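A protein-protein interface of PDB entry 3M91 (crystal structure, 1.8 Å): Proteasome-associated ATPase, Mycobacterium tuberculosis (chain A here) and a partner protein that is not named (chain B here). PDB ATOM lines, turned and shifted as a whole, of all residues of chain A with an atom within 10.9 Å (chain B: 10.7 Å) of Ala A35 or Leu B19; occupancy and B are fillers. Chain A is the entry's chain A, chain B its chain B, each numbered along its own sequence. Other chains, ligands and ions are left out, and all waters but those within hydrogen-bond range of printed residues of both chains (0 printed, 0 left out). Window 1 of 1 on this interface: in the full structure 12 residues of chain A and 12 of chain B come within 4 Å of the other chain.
OE1 of Glu A34 lies close to OE2 of Glu B22.
The side-chain amide nitrogen (NE2) of Gln A38 lies within hydrogen-bond range of the side-chain hydroxyl (OG1) of Thr B16.
OE2 of Glu B22 is in salt-bridge range of NZ of Lys A27 (3.3 Å).
NE2 of Gln A38 sits at hydrogen-bond distance from O of Leu B12 (3.3 Å).
The backbone carbonyl oxygen of Leu B12 sits at hydrogen-bond distance from the side-chain hydroxyl of Thr B16 (2.7 Å).
O of Lys A27 is in hydrogen-bond range of OG1 of Thr A31 (2.7 Å).
Among the printed residues, merely in contact across the chains: Lys A27 with Val B26 (3.6 Å), Leu A28 with Val B26 (3.6 Å), Thr A31 with Glu B22 (3.99 Å), Thr A31 with Ile B23 (3.7 Å), Thr A31 with Val B26 (3.6 Å), Glu A34 with Leu B19 (3.7 Å), Ala A35 with Leu B19 (3.7 Å), Gln A38 with Glu B15 (3.6 Å), Gln A38 with Leu B19 (3.5 Å), Ala A41 with Leu B12 (3.7 Å) and Leu A42 with Thr B16 (3.5 Å).
Of chain B, only Leu B19 (3.7 Å) comes within 4 Å of Ala A35.
Of the printed residues of chain A, Leu B19 touches Glu A34 (3.7 Å), Ala A35 (3.7 Å) and Gln A38 (3.5 Å).
Of chain B, only Leu B12 (3.3 Å), Glu B15 (3.6 Å), Thr B16 (3.0 Å) and Leu B19 (3.5 Å) come within 4 Å of Gln A38.
Of chain A, only Gln A38 and Leu A42 come within 4 Å of Thr B16.
No residue of chain A comes within 4 Å of Asp B18.
Asp B21 touches none of the printed residues of chain A.
Ile B23 touches one residue of chain A.
Printed residues of chain A within 4 Å of Glu B22: Lys A27 (3.3 Å), Thr A31 (3.99 Å) and Glu A34 (3.1 Å).
Printed residues of chain A within 4 Å of Leu B12: Gln A38 (3.3 Å) and Ala A41 (3.7 Å).
Of the printed residues of chain B, Leu A28 touches Val B26 (3.6 Å).
Printed residues of chain A within 4 Å of Val B26: Lys A27, Leu A28 and Thr A31.
Asp B25 touches none of the printed residues of chain A.
Met A29 touches none of the printed residues of chain B.
The nearest residue of chain B that does not touch Ala A35 is Ile B23 (4.4 Å).
The nearest residue of chain A that does not touch Leu B19 is Thr A31 (4.6 Å).
The nearest printed residue of chain A that does not touch Leu B12 is Leu A42 (4.4 Å).
Of the 18 printed residues of chain B, 7 touch a printed residue of chain A.
Hydrophobic or aromatic side chains of chain B within 4 Å of the printed part of chain A: Leu B12, Leu B19, Ile B23 and Val B26.
Of the 18 printed residues of chain A, 8 touch a printed residue of chain B.
Hydrophobic or aromatic side chains of chain A within 4 Å of the printed part of chain B: Leu A28, Ala A41 and Leu A42.
Among the printed residues, Asp or Glu carboxylates within 4 Å of a Lys or Arg side-chain nitrogen of the other chain: Lys A27 with Glu B22 (3.3 Å).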
ATOM      1  N   LYS A  27      16.512 -36.188 -18.874  1.00  0.00           N
ATOM      2  CA  LYS A  27      16.612 -34.744 -18.741  1.00  0.00           C
ATOM      3  C   LYS A  27      15.877 -34.250 -17.470  1.00  0.00           C
ATOM      4  O   LYS A  27      16.367 -33.342 -16.754  1.00  0.00           O
ATOM      5  CB  LYS A  27      16.046 -34.056 -19.984  1.00  0.00           C
ATOM      6  CG  LYS A  27      16.140 -32.534 -19.981  1.00  0.00           C
ATOM      7  CD  LYS A  27      17.626 -32.070 -20.111  1.00  0.00           C
ATOM      8  CE  LYS A  27      17.849 -30.536 -19.839  1.00  0.00           C
ATOM      9  NZ  LYS A  27      19.075 -30.163 -18.988  1.00  0.00           N
ATOM     10  N   LEU A  28      14.715 -34.825 -17.194  1.00  0.00           N
ATOM     11  CA  LEU A  28      13.948 -34.415 -16.068  1.00  0.00           C
ATOM     12  C   LEU A  28      14.699 -34.780 -14.807  1.00  0.00           C
ATOM     13  O   LEU A  28      14.666 -34.018 -13.830  1.00  0.00           O
ATOM     14  CB  LEU A  28      12.551 -35.048 -16.040  1.00  0.00           C
ATOM     15  CG  LEU A  28      11.524 -34.407 -17.005  1.00  0.00           C
ATOM     16  CD1 LEU A  28      10.310 -35.357 -17.146  1.00  0.00           C
ATOM     17  CD2 LEU A  28      11.021 -33.044 -16.608  1.00  0.00           C
ATOM     18  N   MET A  29      15.343 -35.933 -14.821  1.00  0.00           N
ATOM     19  CA  MET A  29      16.056 -36.451 -13.645  1.00  0.00           C
ATOM     20  C   MET A  29      17.302 -35.628 -13.279  1.00  0.00           C
ATOM     21  O   MET A  29      17.579 -35.344 -12.084  1.00  0.00           O
ATOM     22  CB  MET A  29      16.494 -37.889 -13.884  1.00  0.00           C
ATOM     23  CG  MET A  29      16.726 -38.565 -12.573  1.00  0.00           C
ATOM     24  SD  MET A  29      16.842 -40.405 -12.591  1.00  0.00           S
ATOM     25  CE  MET A  29      15.751 -40.860 -13.949  1.00  0.00           C
ATOM     26  N   GLU A  30      18.079 -35.322 -14.311  1.00  0.00           N
ATOM     27  CA  GLU A  30      19.175 -34.399 -14.217  1.00  0.00           C
ATOM     28  C   GLU A  30      18.750 -33.014 -13.651  1.00  0.00           C
ATOM     29  O   GLU A  30      19.476 -32.440 -12.789  1.00  0.00           O
ATOM     30  CB  GLU A  30      19.868 -34.196 -15.580  1.00  0.00           C
ATOM     31  CG  GLU A  30      21.203 -33.354 -15.530  1.00  0.00           C
ATOM     32  CD  GLU A  30      22.199 -33.803 -14.370  1.00  0.00           C
ATOM     33  OE1 GLU A  30      22.587 -35.020 -14.337  1.00  0.00           O
ATOM     34  OE2 GLU A  30      22.576 -32.932 -13.479  1.00  0.00           O
ATOM     35  N   THR A  31      17.658 -32.463 -14.192  1.00  0.00           N
ATOM     36  CA  THR A  31      17.204 -31.134 -13.800  1.00  0.00           C
ATOM     37  C   THR A  31      16.745 -31.209 -12.315  1.00  0.00           C
ATOM     38  O   THR A  31      16.957 -30.291 -11.549  1.00  0.00           O
ATOM     39  CB  THR A  31      16.064 -30.628 -14.692  1.00  0.00           C
ATOM     40  OG1 THR A  31      16.516 -30.704 -16.055  1.00  0.00           O
ATOM     41  CG2 THR A  31      15.822 -29.165 -14.402  1.00  0.00           C
ATOM     42  N   LEU A  32      16.076 -32.296 -11.938  1.00  0.00           N
ATOM     43  CA  LEU A  32      15.650 -32.449 -10.563  1.00  0.00           C
ATOM     44  C   LEU A  32      16.856 -32.616  -9.564  1.00  0.00           C
ATOM     45  O   LEU A  32      16.817 -32.086  -8.413  1.00  0.00           O
ATOM     46  CB  LEU A  32      14.684 -33.655 -10.513  1.00  0.00           C
ATOM     47  CG  LEU A  32      13.825 -33.814  -9.276  1.00  0.00           C
ATOM     48  CD1 LEU A  32      12.935 -32.582  -8.885  1.00  0.00           C
ATOM     49  CD2 LEU A  32      12.960 -35.103  -9.472  1.00  0.00           C
ATOM     50  N   LYS A  33      17.920 -33.299  -9.989  1.00  0.00           N
ATOM     51  CA  LYS A  33      19.127 -33.394  -9.152  1.00  0.00           C
ATOM     52  C   LYS A  33      19.705 -31.986  -8.944  1.00  0.00           C
ATOM     53  O   LYS A  33      20.123 -31.664  -7.857  1.00  0.00           O
ATOM     54  CB  LYS A  33      20.174 -34.237  -9.808  1.00  0.00           C
ATOM     55  CG  LYS A  33      19.959 -35.727  -9.520  1.00  0.00           C
ATOM     56  CD  LYS A  33      20.936 -36.618 -10.357  1.00  0.00           C
ATOM     57  CE  LYS A  33      20.599 -38.100 -10.100  1.00  0.00           C
ATOM     58  NZ  LYS A  33      20.883 -38.961 -11.275  1.00  0.00           N
ATOM     59  N   GLU A  34      19.761 -31.154 -10.005  1.00  0.00           N
ATOM     60  CA  GLU A  34      20.154 -29.782  -9.873  1.00  0.00           C
ATOM     61  C   GLU A  34      19.245 -29.006  -8.924  1.00  0.00           C
ATOM     62  O   GLU A  34      19.764 -28.235  -8.113  1.00  0.00           O
ATOM     63  CB  GLU A  34      20.247 -29.028 -11.217  1.00  0.00           C
ATOM     64  CG  GLU A  34      21.343 -29.694 -12.121  1.00  0.00           C
ATOM     65  CD  GLU A  34      21.283 -29.233 -13.617  1.00  0.00           C
ATOM     66  OE1 GLU A  34      20.467 -28.361 -13.944  1.00  0.00           O
ATOM     67  OE2 GLU A  34      22.063 -29.777 -14.455  1.00  0.00           O
ATOM     68  N   ALA A  35      17.933 -29.209  -8.992  1.00  0.00           N
ATOM     69  CA  ALA A  35      17.014 -28.457  -8.133  1.00  0.00           C
ATOM     70  C   ALA A  35      17.216 -28.896  -6.692  1.00  0.00           C
ATOM     71  O   ALA A  35      17.170 -28.051  -5.763  1.00  0.00           O
ATOM     72  CB  ALA A  35      15.529 -28.736  -8.525  1.00  0.00           C
ATOM     73  N   ARG A  36      17.416 -30.217  -6.487  1.00  0.00           N
ATOM     74  CA  ARG A  36      17.753 -30.746  -5.151  1.00  0.00           C
ATOM     75  C   ARG A  36      18.951 -30.009  -4.506  1.00  0.00           C
ATOM     76  O   ARG A  36      18.800 -29.568  -3.365  1.00  0.00           O
ATOM     77  CB  ARG A  36      17.992 -32.282  -5.226  1.00  0.00           C
ATOM     78  CG  ARG A  36      17.678 -32.982  -3.869  1.00  0.00           C
ATOM     79  CD  ARG A  36      18.930 -33.231  -3.092  1.00  0.00           C
ATOM     80  NE  ARG A  36      18.659 -34.014  -1.855  1.00  0.00           N
ATOM     81  CZ  ARG A  36      19.166 -33.761  -0.629  1.00  0.00           C
ATOM     82  NH1 ARG A  36      20.018 -32.744  -0.392  1.00  0.00           N
ATOM     83  NH2 ARG A  36      18.755 -34.487   0.403  1.00  0.00           N
ATOM     84  N   GLN A  37      20.124 -29.938  -5.181  1.00  0.00           N
ATOM     85  CA  GLN A  37      21.291 -29.228  -4.720  1.00  0.00           C
ATOM     86  C   GLN A  37      21.013 -27.736  -4.455  1.00  0.00           C
ATOM     87  O   GLN A  37      21.489 -27.187  -3.448  1.00  0.00           O
ATOM     88  CB  GLN A  37      22.405 -29.217  -5.791  1.00  0.00           C
ATOM     89  CG  GLN A  37      22.840 -30.631  -6.115  1.00  0.00           C
ATOM     90  CD  GLN A  37      23.998 -30.676  -7.184  1.00  0.00           C
ATOM     91  OE1 GLN A  37      24.851 -29.750  -7.250  1.00  0.00           O
ATOM     92  NE2 GLN A  37      24.008 -31.740  -8.001  1.00  0.00           N
ATOM     93  N   GLN A  38      20.265 -27.072  -5.353  1.00  0.00           N
ATOM     94  CA  GLN A  38      20.029 -25.637  -5.184  1.00  0.00           C
ATOM     95  C   GLN A  38      19.043 -25.436  -4.025  1.00  0.00           C
ATOM     96  O   GLN A  38      19.180 -24.484  -3.291  1.00  0.00           O
ATOM     97  CB  GLN A  38      19.466 -25.045  -6.501  1.00  0.00           C
ATOM     98  CG  GLN A  38      19.425 -23.481  -6.416  1.00  0.00           C
ATOM     99  CD  GLN A  38      20.872 -22.939  -6.334  1.00  0.00           C
ATOM    100  OE1 GLN A  38      21.774 -23.636  -6.666  1.00  0.00           O
ATOM    101  NE2 GLN A  38      21.052 -21.791  -5.816  1.00  0.00           N
ATOM    102  N   LEU A  39      18.038 -26.296  -3.860  1.00  0.00           N
ATOM    103  CA  LEU A  39      17.157 -26.138  -2.720  1.00  0.00           C
ATOM    104  C   LEU A  39      17.934 -26.213  -1.386  1.00  0.00           C
ATOM    105  O   LEU A  39      17.620 -25.502  -0.423  1.00  0.00           O
ATOM    106  CB  LEU A  39      16.076 -27.225  -2.669  1.00  0.00           C
ATOM    107  CG  LEU A  39      14.906 -27.102  -3.682  1.00  0.00           C
ATOM    108  CD1 LEU A  39      14.198 -28.513  -3.942  1.00  0.00           C
ATOM    109  CD2 LEU A  39      13.946 -25.964  -3.337  1.00  0.00           C
ATOM    110  N   LEU A  40      18.855 -27.182  -1.306  1.00  0.00           N
ATOM    111  CA  LEU A  40      19.632 -27.331  -0.105  1.00  0.00           C
ATOM    112  C   LEU A  40      20.471 -26.066   0.098  1.00  0.00           C
ATOM    113  O   LEU A  40      20.604 -25.576   1.238  1.00  0.00           O
ATOM    114  CB  LEU A  40      20.500 -28.594  -0.237  1.00  0.00           C
ATOM    115  CG  LEU A  40      21.425 -28.925   0.934  1.00  0.00           C
ATOM    116  CD1 LEU A  40      20.527 -29.242   2.198  1.00  0.00           C
ATOM    117  CD2 LEU A  40      22.429 -30.126   0.633  1.00  0.00           C
ATOM    118  N   ALA A  41      21.122 -25.579  -0.952  1.00  0.00           N
ATOM    119  CA  ALA A  41      21.972 -24.371  -0.778  1.00  0.00           C
ATOM    120  C   ALA A  41      21.139 -23.156  -0.320  1.00  0.00           C
ATOM    121  O   ALA A  41      21.585 -22.395   0.529  1.00  0.00           O
ATOM    122  CB  ALA A  41      22.754 -24.047  -2.102  1.00  0.00           C
ATOM    123  N   LEU A  42      19.902 -23.051  -0.811  1.00  0.00           N
ATOM    124  CA  LEU A  42      19.059 -21.919  -0.394  1.00  0.00           C
ATOM    125  C   LEU A  42      18.576 -22.120   1.023  1.00  0.00           C
ATOM    126  O   LEU A  42      18.608 -21.193   1.792  1.00  0.00           O
ATOM    127  CB  LEU A  42      17.847 -21.758  -1.299  1.00  0.00           C
ATOM    128  CG  LEU A  42      18.244 -21.152  -2.696  1.00  0.00           C
ATOM    129  CD1 LEU A  42      17.054 -21.417  -3.704  1.00  0.00           C
ATOM    130  CD2 LEU A  42      18.583 -19.637  -2.642  1.00  0.00           C
ATOM    131  N   ARG A  43      18.213 -23.363   1.359  1.00  0.00           N
ATOM    132  CA  ARG A  43      17.812 -23.609   2.792  1.00  0.00           C
ATOM    133  C   ARG A  43      18.980 -23.256   3.733  1.00  0.00           C
ATOM    134  O   ARG A  43      18.762 -22.655   4.767  1.00  0.00           O
ATOM    135  CB  ARG A  43      17.437 -25.071   2.944  1.00  0.00           C
ATOM    136  CG  ARG A  43      16.736 -25.321   4.353  1.00  0.00           C
ATOM    137  CD  ARG A  43      16.811 -26.870   4.718  1.00  0.00           C
ATOM    138  NE  ARG A  43      18.159 -27.230   5.134  1.00  0.00           N
ATOM    139  CZ  ARG A  43      18.658 -28.458   5.151  1.00  0.00           C
ATOM    140  NH1 ARG A  43      17.927 -29.506   4.844  1.00  0.00           N
ATOM    141  NH2 ARG A  43      19.950 -28.626   5.500  1.00  0.00           N
ATOM    142  N   GLU A  44      20.228 -23.615   3.437  1.00  0.00           N
ATOM    143  CA  GLU A  44      21.368 -23.257   4.293  1.00  0.00           C
ATOM    144  C   GLU A  44      21.569 -21.723   4.420  1.00  0.00           C
ATOM    145  O   GLU A  44      21.882 -21.209   5.513  1.00  0.00           O
ATOM    146  CB  GLU A  44      22.660 -23.858   3.684  1.00  0.00           C
ATOM    147  CG  GLU A  44      22.636 -25.381   3.629  1.00  0.00           C
ATOM    148  CD  GLU A  44      22.943 -26.019   4.974  1.00  0.00           C
ATOM    149  OE1 GLU A  44      23.617 -25.394   5.843  1.00  0.00           O
ATOM    150  OE2 GLU A  44      22.560 -27.207   5.145  1.00  0.00           O
ATOM    151  N   LYS B  11      25.384 -14.418  -5.536  1.00  0.00           N
ATOM    152  CA  LYS B  11      25.730 -15.576  -6.330  1.00  0.00           C
ATOM    153  C   LYS B  11      24.605 -16.656  -6.292  1.00  0.00           C
ATOM    154  O   LYS B  11      24.266 -17.277  -7.308  1.00  0.00           O
ATOM    155  CB  LYS B  11      27.097 -16.166  -5.877  1.00  0.00           C
ATOM    156  CG  LYS B  11      28.313 -15.355  -6.311  1.00  0.00           C
ATOM    157  CD  LYS B  11      29.541 -16.151  -5.854  1.00  0.00           C
ATOM    158  CE  LYS B  11      30.732 -15.710  -6.604  1.00  0.00           C
ATOM    159  NZ  LYS B  11      31.924 -16.034  -5.836  1.00  0.00           N
ATOM    160  N   LEU B  12      24.049 -16.908  -5.121  1.00  0.00           N
ATOM    161  CA  LEU B  12      23.085 -17.946  -4.913  1.00  0.00           C
ATOM    162  C   LEU B  12      21.768 -17.591  -5.604  1.00  0.00           C
ATOM    163  O   LEU B  12      21.142 -18.480  -6.184  1.00  0.00           O
ATOM    164  CB  LEU B  12      22.771 -18.024  -3.412  1.00  0.00           C
ATOM    165  CG  LEU B  12      23.396 -19.117  -2.661  1.00  0.00           C
ATOM    166  CD1 LEU B  12      22.951 -18.832  -1.148  1.00  0.00           C
ATOM    167  CD2 LEU B  12      22.864 -20.471  -3.172  1.00  0.00           C
ATOM    168  N   THR B  13      21.317 -16.368  -5.492  1.00  0.00           N
ATOM    169  CA  THR B  13      20.108 -15.967  -6.184  1.00  0.00           C
ATOM    170  C   THR B  13      20.253 -15.977  -7.703  1.00  0.00           C
ATOM    171  O   THR B  13      19.353 -16.321  -8.394  1.00  0.00           O
ATOM    172  CB  THR B  13      19.532 -14.642  -5.703  1.00  0.00           C
ATOM    173  OG1 THR B  13      20.478 -13.624  -5.853  1.00  0.00           O
ATOM    174  CG2 THR B  13      19.145 -14.749  -4.260  1.00  0.00           C
ATOM    175  N   GLU B  14      21.406 -15.559  -8.179  1.00  0.00           N
ATOM    176  CA  GLU B  14      21.666 -15.583  -9.601  1.00  0.00           C
ATOM    177  C   GLU B  14      21.698 -17.011 -10.121  1.00  0.00           C
ATOM    178  O   GLU B  14      21.096 -17.270 -11.104  1.00  0.00           O
ATOM    179  CB  GLU B  14      22.910 -14.784  -9.937  1.00  0.00           C
ATOM    180  CG  GLU B  14      23.559 -15.093 -11.258  1.00  0.00           C
ATOM    181  CD  GLU B  14      22.686 -14.896 -12.483  1.00  0.00           C
ATOM    182  OE1 GLU B  14      21.788 -14.010 -12.521  1.00  0.00           O
ATOM    183  OE2 GLU B  14      22.927 -15.660 -13.451  1.00  0.00           O
ATOM    184  N   GLU B  15      22.344 -17.938  -9.415  1.00  0.00           N
ATOM    185  CA  GLU B  15      22.260 -19.334  -9.806  1.00  0.00           C
ATOM    186  C   GLU B  15      20.849 -19.857  -9.745  1.00  0.00           C
ATOM    187  O   GLU B  15      20.489 -20.688 -10.582  1.00  0.00           O
ATOM    188  CB  GLU B  15      23.051 -20.275  -8.863  1.00  0.00           C
ATOM    189  CG  GLU B  15      24.393 -19.789  -8.675  1.00  0.00           C
ATOM    190  CD  GLU B  15      25.147 -20.574  -7.553  1.00  0.00           C
ATOM    191  OE1 GLU B  15      24.494 -21.232  -6.645  1.00  0.00           O
ATOM    192  OE2 GLU B  15      26.399 -20.525  -7.629  1.00  0.00           O
ATOM    193  N   THR B  16      20.101 -19.473  -8.728  1.00  0.00           N
ATOM    194  CA  THR B  16      18.708 -19.930  -8.623  1.00  0.00           C
ATOM    195  C   THR B  16      17.943 -19.413  -9.891  1.00  0.00           C
ATOM    196  O   THR B  16      17.154 -20.149 -10.441  1.00  0.00           O
ATOM    197  CB  THR B  16      18.084 -19.372  -7.371  1.00  0.00           C
ATOM    198  OG1 THR B  16      18.872 -19.850  -6.253  1.00  0.00           O
ATOM    199  CG2 THR B  16      16.565 -19.862  -7.218  1.00  0.00           C
ATOM    200  N   ASP B  17      18.161 -18.162 -10.290  1.00  0.00           N
ATOM    201  CA  ASP B  17      17.435 -17.636 -11.477  1.00  0.00           C
ATOM    202  C   ASP B  17      17.778 -18.422 -12.743  1.00  0.00           C
ATOM    203  O   ASP B  17      16.870 -18.718 -13.525  1.00  0.00           O
ATOM    204  CB  ASP B  17      17.758 -16.147 -11.661  1.00  0.00           C
ATOM    205  CG  ASP B  17      17.240 -15.287 -10.512  1.00  0.00           C
ATOM    206  OD1 ASP B  17      16.216 -15.631  -9.876  1.00  0.00           O
ATOM    207  OD2 ASP B  17      17.771 -14.167 -10.324  1.00  0.00           O
ATOM    208  N   ASP B  18      19.054 -18.751 -12.954  1.00  0.00           N
ATOM    209  CA  ASP B  18      19.470 -19.544 -14.133  1.00  0.00           C
ATOM    210  C   ASP B  18      18.756 -20.892 -14.095  1.00  0.00           C
ATOM    211  O   ASP B  18      18.267 -21.359 -15.124  1.00  0.00           O
ATOM    212  CB  ASP B  18      20.966 -19.846 -14.148  1.00  0.00           C
ATOM    213  CG  ASP B  18      21.835 -18.598 -14.483  1.00  0.00           C
ATOM    214  OD1 ASP B  18      21.298 -17.637 -15.077  1.00  0.00           O
ATOM    215  OD2 ASP B  18      23.043 -18.557 -14.097  1.00  0.00           O
ATOM    216  N   LEU B  19      18.633 -21.487 -12.911  1.00  0.00           N
ATOM    217  CA  LEU B  19      17.954 -22.809 -12.782  1.00  0.00           C
ATOM    218  C   LEU B  19      16.457 -22.664 -12.961  1.00  0.00           C
ATOM    219  O   LEU B  19      15.867 -23.589 -13.552  1.00  0.00           O
ATOM    220  CB  LEU B  19      18.182 -23.417 -11.375  1.00  0.00           C
ATOM    221  CG  LEU B  19      17.648 -24.831 -11.162  1.00  0.00           C
ATOM    222  CD1 LEU B  19      18.142 -25.831 -12.285  1.00  0.00           C
ATOM    223  CD2 LEU B  19      18.160 -25.278  -9.718  1.00  0.00           C
ATOM    224  N   LEU B  20      15.842 -21.586 -12.472  1.00  0.00           N
ATOM    225  CA  LEU B  20      14.400 -21.389 -12.668  1.00  0.00           C
ATOM    226  C   LEU B  20      14.114 -21.310 -14.210  1.00  0.00           C
ATOM    227  O   LEU B  20      13.152 -21.939 -14.701  1.00  0.00           O
ATOM    228  CB  LEU B  20      13.895 -20.112 -12.041  1.00  0.00           C
ATOM    229  CG  LEU B  20      13.864 -20.246 -10.465  1.00  0.00           C
ATOM    230  CD1 LEU B  20      13.590 -18.853  -9.874  1.00  0.00           C
ATOM    231  CD2 LEU B  20      12.841 -21.284 -10.141  1.00  0.00           C
ATOM    232  N   ASP B  21      14.928 -20.546 -14.951  1.00  0.00           N
ATOM    233  CA  ASP B  21      14.693 -20.403 -16.407  1.00  0.00           C
ATOM    234  C   ASP B  21      14.872 -21.769 -17.065  1.00  0.00           C
ATOM    235  O   ASP B  21      14.113 -22.095 -17.978  1.00  0.00           O
ATOM    236  CB  ASP B  21      15.780 -19.481 -16.972  1.00  0.00           C
ATOM    237  CG  ASP B  21      15.573 -18.037 -16.634  1.00  0.00           C
ATOM    238  OD1 ASP B  21      14.498 -17.668 -16.133  1.00  0.00           O
ATOM    239  OD2 ASP B  21      16.512 -17.242 -16.863  1.00  0.00           O
ATOM    240  N   GLU B  22      15.883 -22.565 -16.640  1.00  0.00           N
ATOM    241  CA  GLU B  22      16.118 -23.866 -17.203  1.00  0.00           C
ATOM    242  C   GLU B  22      14.985 -24.866 -16.892  1.00  0.00           C
ATOM    243  O   GLU B  22      14.585 -25.684 -17.774  1.00  0.00           O
ATOM    244  CB  GLU B  22      17.372 -24.484 -16.619  1.00  0.00           C
ATOM    245  CG  GLU B  22      17.735 -25.810 -17.250  1.00  0.00           C
ATOM    246  CD  GLU B  22      18.970 -26.484 -16.584  1.00  0.00           C
ATOM    247  OE1 GLU B  22      19.802 -25.746 -15.972  1.00  0.00           O
ATOM    248  OE2 GLU B  22      19.111 -27.744 -16.681  1.00  0.00           O
ATOM    249  N   ILE B  23      14.514 -24.847 -15.646  1.00  0.00           N
ATOM    250  CA  ILE B  23      13.327 -25.605 -15.269  1.00  0.00           C
ATOM    251  C   ILE B  23      12.107 -25.270 -16.193  1.00  0.00           C
ATOM    252  O   ILE B  23      11.446 -26.209 -16.700  1.00  0.00           O
ATOM    253  CB  ILE B  23      13.002 -25.387 -13.826  1.00  0.00           C
ATOM    254  CG1 ILE B  23      14.058 -26.188 -13.017  1.00  0.00           C
ATOM    255  CG2 ILE B  23      11.634 -26.051 -13.485  1.00  0.00           C
ATOM    256  CD1 ILE B  23      13.971 -25.908 -11.486  1.00  0.00           C
ATOM    257  N   ASP B  24      11.831 -23.983 -16.394  1.00  0.00           N
ATOM    258  CA  ASP B  24      10.710 -23.565 -17.224  1.00  0.00           C
ATOM    259  C   ASP B  24      10.881 -24.081 -18.657  1.00  0.00           C
ATOM    260  O   ASP B  24       9.906 -24.589 -19.250  1.00  0.00           O
ATOM    261  CB  ASP B  24      10.611 -22.052 -17.242  1.00  0.00           C
ATOM    262  CG  ASP B  24      10.188 -21.493 -15.889  1.00  0.00           C
ATOM    263  OD1 ASP B  24       9.723 -22.259 -15.014  1.00  0.00           O
ATOM    264  OD2 ASP B  24      10.333 -20.269 -15.646  1.00  0.00           O
ATOM    265  N   ASP B  25      12.101 -23.998 -19.198  1.00  0.00           N
ATOM    266  CA  ASP B  25      12.406 -24.576 -20.507  1.00  0.00           C
ATOM    267  C   ASP B  25      12.139 -26.103 -20.576  1.00  0.00           C
ATOM    268  O   ASP B  25      11.532 -26.584 -21.545  1.00  0.00           O
ATOM    269  CB  ASP B  25      13.882 -24.333 -20.882  1.00  0.00           C
ATOM    270  CG  ASP B  25      14.219 -22.833 -21.200  1.00  0.00           C
ATOM    271  OD1 ASP B  25      13.302 -21.977 -21.411  1.00  0.00           O
ATOM    272  OD2 ASP B  25      15.451 -22.511 -21.285  1.00  0.00           O
ATOM    273  N   VAL B  26      12.693 -26.864 -19.620  1.00  0.00           N
ATOM    274  CA  VAL B  26      12.495 -28.298 -19.470  1.00  0.00           C
ATOM    275  C   VAL B  26      10.995 -28.667 -19.408  1.00  0.00           C
ATOM    276  O   VAL B  26      10.519 -29.610 -20.131  1.00  0.00           O
ATOM    277  CB  VAL B  26      13.346 -28.839 -18.261  1.00  0.00           C
ATOM    278  CG1 VAL B  26      12.962 -30.260 -17.877  1.00  0.00           C
ATOM    279  CG2 VAL B  26      14.834 -28.867 -18.689  1.00  0.00           C
ATOM    280  N   LEU B  27      10.252 -27.907 -18.628  1.00  0.00           N
ATOM    281  CA  LEU B  27       8.871 -28.208 -18.398  1.00  0.00           C
ATOM    282  C   LEU B  27       8.040 -27.893 -19.658  1.00  0.00           C
ATOM    283  O   LEU B  27       7.122 -28.655 -19.984  1.00  0.00           O
ATOM    284  CB  LEU B  27       8.345 -27.440 -17.200  1.00  0.00           C
ATOM    285  CG  LEU B  27       8.794 -27.935 -15.814  1.00  0.00           C
ATOM    286  CD1 LEU B  27       8.280 -26.991 -14.818  1.00  0.00           C
ATOM    287  CD2 LEU B  27       8.314 -29.326 -15.509  1.00  0.00           C
ATOM    288  N   GLU B  28       8.354 -26.809 -20.372  1.00  0.00           N
ATOM    289  CA  GLU B  28       7.675 -26.524 -21.655  1.00  0.00           C
ATOM    290  C   GLU B  28       8.090 -27.515 -22.771  1.00  0.00           C
ATOM    291  O   GLU B  28       7.241 -27.898 -23.568  1.00  0.00           O
ATOM    292  CB  GLU B  28       7.878 -25.068 -22.112  1.00  0.00           C
ATOM    293  CG  GLU B  28       9.037 -24.875 -23.144  1.00  0.00           C
ATOM    294  CD  GLU B  28       9.197 -23.429 -23.666  1.00  0.00           C
ATOM    295  OE1 GLU B  28       8.203 -22.849 -24.214  1.00  0.00           O
ATOM    296  OE2 GLU B  28      10.339 -22.882 -23.548  1.00  0.00           O
